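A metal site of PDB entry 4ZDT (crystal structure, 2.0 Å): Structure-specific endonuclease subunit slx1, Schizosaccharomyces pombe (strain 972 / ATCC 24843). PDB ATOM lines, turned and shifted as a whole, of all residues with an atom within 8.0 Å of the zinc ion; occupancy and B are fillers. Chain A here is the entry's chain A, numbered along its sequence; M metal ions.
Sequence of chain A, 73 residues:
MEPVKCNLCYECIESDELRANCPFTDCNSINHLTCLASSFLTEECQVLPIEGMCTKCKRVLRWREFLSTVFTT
O of Ser 29 is in hydrogen-bond range of N of Cys 22 (3.0 Å).
The side-chain sulfur of Cys 57 lies close to the guanidinium group of Arg 59, 3.4 Å away.
The backbone NH (N) of Cys 54 sits at hydrogen-bond distance from the backbone carbonyl oxygen (O) of Arg 59.
The side-chain sulfur (SG) of Cys 54 lies close to the backbone NH (N) of Lys 56 (3.6 Å).
The side-chain sulfur (SG) of Cys 27 lies close to the backbone NH (N) of Ser 29.
The side-chain amino group (NZ) of Lys 56 lies within hydrogen-bond range of the backbone carbonyl oxygen (O) of Cys 27, at 2.8 Å.
The zinc ion is bound by SG of Cys 22 (2.3 Å), SG of Cys 57 (2.3 Å), SG of Cys 54 (2.4 Å) and SG of Cys 27 (2.4 Å).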
ATOM      1  N   ASN A   7      -4.546   5.600  15.517  1.00  0.00           N
ATOM      2  CA  ASN A   7      -3.276   6.232  15.162  1.00  0.00           C
ATOM      3  C   ASN A   7      -3.027   6.410  13.665  1.00  0.00           C
ATOM      4  O   ASN A   7      -1.918   6.752  13.256  1.00  0.00           O
ATOM      5  CB  ASN A   7      -2.112   5.464  15.795  1.00  0.00           C
ATOM      6  CG  ASN A   7      -1.861   4.132  15.117  1.00  0.00           C
ATOM      7  OD1 ASN A   7      -2.726   3.597  14.422  1.00  0.00           O
ATOM      8  ND2 ASN A   7      -0.664   3.582  15.300  1.00  0.00           N
ATOM      9  N   ASN A  21      -4.090  -3.772  17.700  1.00  0.00           N
ATOM     10  CA  ASN A  21      -2.974  -3.299  18.506  1.00  0.00           C
ATOM     11  C   ASN A  21      -1.718  -4.129  18.246  1.00  0.00           C
ATOM     12  O   ASN A  21      -1.775  -5.360  18.156  1.00  0.00           O
ATOM     13  CB  ASN A  21      -3.294  -3.262  20.004  1.00  0.00           C
ATOM     14  CG  ASN A  21      -3.251  -4.628  20.636  1.00  0.00           C
ATOM     15  OD1 ASN A  21      -4.149  -5.462  20.411  1.00  0.00           O
ATOM     16  ND2 ASN A  21      -2.199  -4.888  21.408  1.00  0.00           N
ATOM     17  N   CYS A  22      -0.597  -3.436  18.117  1.00  0.00           N
ATOM     18  CA  CYS A  22       0.696  -4.080  18.053  1.00  0.00           C
ATOM     19  C   CYS A  22       0.852  -4.871  19.357  1.00  0.00           C
ATOM     20  O   CYS A  22       0.657  -4.327  20.440  1.00  0.00           O
ATOM     21  CB  CYS A  22       1.802  -3.050  17.895  1.00  0.00           C
ATOM     22  SG  CYS A  22       3.466  -3.747  17.735  1.00  0.00           S
ATOM     23  N   PRO A  23       1.192  -6.171  19.244  1.00  0.00           N
ATOM     24  CA  PRO A  23       1.195  -7.040  20.426  1.00  0.00           C
ATOM     25  C   PRO A  23       2.359  -6.785  21.378  1.00  0.00           C
ATOM     26  O   PRO A  23       2.393  -7.401  22.424  1.00  0.00           O
ATOM     27  CB  PRO A  23       1.293  -8.471  19.823  1.00  0.00           C
ATOM     28  CG  PRO A  23       2.046  -8.271  18.523  1.00  0.00           C
ATOM     29  CD  PRO A  23       1.597  -6.886  18.006  1.00  0.00           C
ATOM     30  N   PHE A  24       3.289  -5.908  21.009  1.00  0.00           N
ATOM     31  CA  PHE A  24       4.412  -5.606  21.890  1.00  0.00           C
ATOM     32  C   PHE A  24       4.060  -4.401  22.780  1.00  0.00           C
ATOM     33  O   PHE A  24       3.758  -3.322  22.301  1.00  0.00           O
ATOM     34  CB  PHE A  24       5.710  -5.378  21.088  1.00  0.00           C
ATOM     35  CG  PHE A  24       6.190  -6.630  20.384  1.00  0.00           C
ATOM     36  CD1 PHE A  24       5.714  -6.959  19.116  1.00  0.00           C
ATOM     37  CD2 PHE A  24       7.034  -7.523  21.036  1.00  0.00           C
ATOM     38  CE1 PHE A  24       6.145  -8.158  18.452  1.00  0.00           C
ATOM     39  CE2 PHE A  24       7.450  -8.723  20.411  1.00  0.00           C
ATOM     40  CZ  PHE A  24       7.004  -9.038  19.126  1.00  0.00           C
ATOM     41  N   THR A  25       4.101  -4.626  24.081  1.00  0.00           N
ATOM     42  CA  THR A  25       3.736  -3.600  25.069  1.00  0.00           C
ATOM     43  C   THR A  25       4.653  -2.384  24.956  1.00  0.00           C
ATOM     44  O   THR A  25       4.230  -1.261  25.238  1.00  0.00           O
ATOM     45  CB  THR A  25       3.723  -4.170  26.469  1.00  0.00           C
ATOM     46  OG1 THR A  25       2.924  -5.351  26.453  1.00  0.00           O
ATOM     47  CG2 THR A  25       3.092  -3.197  27.476  1.00  0.00           C
ATOM     48  N   ASP A  26       5.893  -2.586  24.484  1.00  0.00           N
ATOM     49  CA  ASP A  26       6.810  -1.472  24.294  1.00  0.00           C
ATOM     50  C   ASP A  26       6.361  -0.536  23.180  1.00  0.00           C
ATOM     51  O   ASP A  26       6.899   0.554  23.037  1.00  0.00           O
ATOM     52  CB  ASP A  26       8.285  -1.914  24.097  1.00  0.00           C
ATOM     53  CG  ASP A  26       8.537  -2.689  22.776  1.00  0.00           C
ATOM     54  OD1 ASP A  26       7.911  -2.365  21.730  1.00  0.00           O
ATOM     55  OD2 ASP A  26       9.392  -3.591  22.776  1.00  0.00           O
ATOM     56  N   CYS A  27       5.366  -0.976  22.413  1.00  0.00           N
ATOM     57  CA  CYS A  27       4.871  -0.193  21.291  1.00  0.00           C
ATOM     58  C   CYS A  27       3.379   0.118  21.475  1.00  0.00           C
ATOM     59  O   CYS A  27       2.996   1.277  21.605  1.00  0.00           O
ATOM     60  CB  CYS A  27       5.090  -0.949  19.984  1.00  0.00           C
ATOM     61  SG  CYS A  27       4.298  -0.137  18.598  1.00  0.00           S
ATOM     62  N   ASN A  28       2.559  -0.944  21.485  1.00  0.00           N
ATOM     63  CA  ASN A  28       1.118  -0.861  21.712  1.00  0.00           C
ATOM     64  C   ASN A  28       0.395   0.136  20.783  1.00  0.00           C
ATOM     65  O   ASN A  28      -0.550   0.793  21.200  1.00  0.00           O
ATOM     66  CB  ASN A  28       0.823  -0.562  23.209  1.00  0.00           C
ATOM     67  CG  ASN A  28      -0.600  -0.872  23.607  1.00  0.00           C
ATOM     68  OD1 ASN A  28      -1.144  -1.910  23.234  1.00  0.00           O
ATOM     69  ND2 ASN A  28      -1.225   0.026  24.357  1.00  0.00           N
ATOM     70  N   SER A  29       0.854   0.243  19.533  1.00  0.00           N
ATOM     71  CA  SER A  29       0.188   1.048  18.503  1.00  0.00           C
ATOM     72  C   SER A  29      -1.263   0.590  18.292  1.00  0.00           C
ATOM     73  O   SER A  29      -1.485  -0.581  17.947  1.00  0.00           O
ATOM     74  CB  SER A  29       0.945   0.927  17.186  1.00  0.00           C
ATOM     75  OG  SER A  29       0.287   1.657  16.159  1.00  0.00           O
ATOM     76  N   ILE A  30      -2.216   1.494  18.499  1.00  0.00           N
ATOM     77  CA  ILE A  30      -3.640   1.160  18.417  1.00  0.00           C
ATOM     78  C   ILE A  30      -4.277   1.829  17.188  1.00  0.00           C
ATOM     79  O   ILE A  30      -3.999   2.998  16.880  1.00  0.00           O
ATOM     80  CB  ILE A  30      -4.395   1.471  19.735  1.00  0.00           C
ATOM     81  CG1 ILE A  30      -3.853   0.563  20.873  1.00  0.00           C
ATOM     82  CG2 ILE A  30      -5.901   1.223  19.598  1.00  0.00           C
ATOM     83  CD1 ILE A  30      -4.282   0.970  22.290  1.00  0.00           C
ATOM     84  N   MET A  53       4.214  -3.736   8.276  1.00  0.00           N
ATOM     85  CA  MET A  53       5.121  -3.089   9.203  1.00  0.00           C
ATOM     86  C   MET A  53       4.326  -2.193  10.151  1.00  0.00           C
ATOM     87  O   MET A  53       3.594  -1.316   9.689  1.00  0.00           O
ATOM     88  CB  MET A  53       6.141  -2.242   8.459  1.00  0.00           C
ATOM     89  CG  MET A  53       7.153  -1.569   9.381  1.00  0.00           C
ATOM     90  SD  MET A  53       8.264  -0.448   8.521  1.00  0.00           S
ATOM     91  CE  MET A  53       9.502  -1.598   7.921  1.00  0.00           C
ATOM     92  N   CYS A  54       4.453  -2.424  11.453  1.00  0.00           N
ATOM     93  CA  CYS A  54       3.871  -1.504  12.419  1.00  0.00           C
ATOM     94  C   CYS A  54       4.508  -0.123  12.236  1.00  0.00           C
ATOM     95  O   CYS A  54       5.736   0.021  12.258  1.00  0.00           O
ATOM     96  CB  CYS A  54       4.100  -2.001  13.842  1.00  0.00           C
ATOM     97  SG  CYS A  54       3.435  -0.868  15.107  1.00  0.00           S
ATOM     98  N   THR A  55       3.693   0.913  12.046  1.00  0.00           N
ATOM     99  CA  THR A  55       4.258   2.235  11.736  1.00  0.00           C
ATOM    100  C   THR A  55       4.992   2.879  12.927  1.00  0.00           C
ATOM    101  O   THR A  55       5.844   3.754  12.740  1.00  0.00           O
ATOM    102  CB  THR A  55       3.201   3.186  11.136  1.00  0.00           C
ATOM    103  OG1 THR A  55       3.884   4.257  10.474  1.00  0.00           O
ATOM    104  CG2 THR A  55       2.304   3.755  12.201  1.00  0.00           C
ATOM    105  N   LYS A  56       4.672   2.412  14.127  1.00  0.00           N
ATOM    106  CA  LYS A  56       5.257   2.950  15.348  1.00  0.00           C
ATOM    107  C   LYS A  56       6.600   2.258  15.651  1.00  0.00           C
ATOM    108  O   LYS A  56       7.648   2.905  15.612  1.00  0.00           O
ATOM    109  CB  LYS A  56       4.235   2.895  16.510  1.00  0.00           C
ATOM    110  CG  LYS A  56       4.653   3.654  17.793  1.00  0.00           C
ATOM    111  CD  LYS A  56       3.654   3.482  18.953  1.00  0.00           C
ATOM    112  CE  LYS A  56       4.084   4.303  20.204  1.00  0.00           C
ATOM    113  NZ  LYS A  56       3.180   4.098  21.383  1.00  0.00           N
ATOM    114  N   CYS A  57       6.603   0.929  15.883  1.00  0.00           N
ATOM    115  CA  CYS A  57       7.857   0.214  16.209  1.00  0.00           C
ATOM    116  C   CYS A  57       8.676  -0.321  15.019  1.00  0.00           C
ATOM    117  O   CYS A  57       9.817  -0.762  15.200  1.00  0.00           O
ATOM    118  CB  CYS A  57       7.580  -0.926  17.202  1.00  0.00           C
ATOM    119  SG  CYS A  57       6.675  -2.319  16.434  1.00  0.00           S
ATOM    120  N   LYS A  58       8.095  -0.308  13.820  1.00  0.00           N
ATOM    121  CA  LYS A  58       8.759  -0.812  12.597  1.00  0.00           C
ATOM    122  C   LYS A  58       8.980  -2.329  12.527  1.00  0.00           C
ATOM    123  O   LYS A  58       9.671  -2.785  11.635  1.00  0.00           O
ATOM    124  CB  LYS A  58      10.119  -0.117  12.322  1.00  0.00           C
ATOM    125  CG  LYS A  58      10.125   1.392  12.475  1.00  0.00           C
ATOM    126  CD  LYS A  58       9.110   2.080  11.577  1.00  0.00           C
ATOM    127  CE  LYS A  58       9.285   3.592  11.655  1.00  0.00           C
ATOM    128  NZ  LYS A  58       8.188   4.285  10.949  1.00  0.00           N
ATOM    129  N   ARG A  59       8.423  -3.105  13.456  1.00  0.00           N
ATOM    130  CA  ARG A  59       8.495  -4.569  13.316  1.00  0.00           C
ATOM    131  C   ARG A  59       7.582  -4.994  12.160  1.00  0.00           C
ATOM    132  O   ARG A  59       6.574  -4.334  11.899  1.00  0.00           O
ATOM    133  CB  ARG A  59       8.049  -5.275  14.593  1.00  0.00           C
ATOM    134  CG  ARG A  59       8.981  -5.086  15.821  1.00  0.00           C
ATOM    135  CD  ARG A  59       8.302  -5.715  17.035  1.00  0.00           C
ATOM    136  NE  ARG A  59       9.098  -5.731  18.268  1.00  0.00           N
ATOM    137  CZ  ARG A  59       8.992  -4.842  19.245  1.00  0.00           C
ATOM    138  NH1 ARG A  59       8.140  -3.797  19.132  1.00  0.00           N
ATOM    139  NH2 ARG A  59       9.732  -4.968  20.343  1.00  0.00           N
ATOM    140  N   VAL A  60       7.937  -6.083  11.464  1.00  0.00           N
ATOM    141  CA  VAL A  60       7.098  -6.592  10.359  1.00  0.00           C
ATOM    142  C   VAL A  60       6.449  -7.865  10.829  1.00  0.00           C
ATOM    143  O   VAL A  60       7.135  -8.885  11.026  1.00  0.00           O
ATOM    144  CB  VAL A  60       7.893  -6.825   9.059  1.00  0.00           C
ATOM    145  CG1 VAL A  60       7.004  -7.435   7.982  1.00  0.00           C
ATOM    146  CG2 VAL A  60       8.482  -5.509   8.566  1.00  0.00           C
ATOM    147  N   LEU A  61       5.134  -7.810  11.022  1.00  0.00           N
ATOM    148  CA  LEU A  61       4.400  -8.885  11.672  1.00  0.00           C
ATOM    149  C   LEU A  61       3.294  -9.372  10.777  1.00  0.00           C
ATOM    150  O   LEU A  61       2.908  -8.677   9.843  1.00  0.00           O
ATOM    151  CB  LEU A  61       3.813  -8.399  13.001  1.00  0.00           C
ATOM    152  CG  LEU A  61       4.839  -7.757  13.955  1.00  0.00           C
ATOM    153  CD1 LEU A  61       4.070  -7.157  15.128  1.00  0.00           C
ATOM    154  CD2 LEU A  61       5.862  -8.784  14.438  1.00  0.00           C
ATOM    155  N   PHE A  66      -1.839  -8.650  15.134  1.00  0.00           N
ATOM    156  CA  PHE A  66      -2.499  -7.404  15.533  1.00  0.00           C
ATOM    157  C   PHE A  66      -3.878  -7.628  16.145  1.00  0.00           C
ATOM    158  O   PHE A  66      -4.528  -6.677  16.607  1.00  0.00           O
ATOM    159  CB  PHE A  66      -2.543  -6.422  14.368  1.00  0.00           C
ATOM    160  CG  PHE A  66      -1.188  -6.015  13.880  1.00  0.00           C
ATOM    161  CD1 PHE A  66      -0.505  -4.960  14.498  1.00  0.00           C
ATOM    162  CD2 PHE A  66      -0.588  -6.664  12.790  1.00  0.00           C
ATOM    163  CE1 PHE A  66       0.749  -4.568  14.042  1.00  0.00           C
ATOM    164  CE2 PHE A  66       0.665  -6.282  12.331  1.00  0.00           C
ATOM    165  CZ  PHE A  66       1.338  -5.225  12.978  1.00  0.00           C
HETATM  166 ZN    ZN M   1       4.469  -1.854  16.983  1.00  0.00          ZN
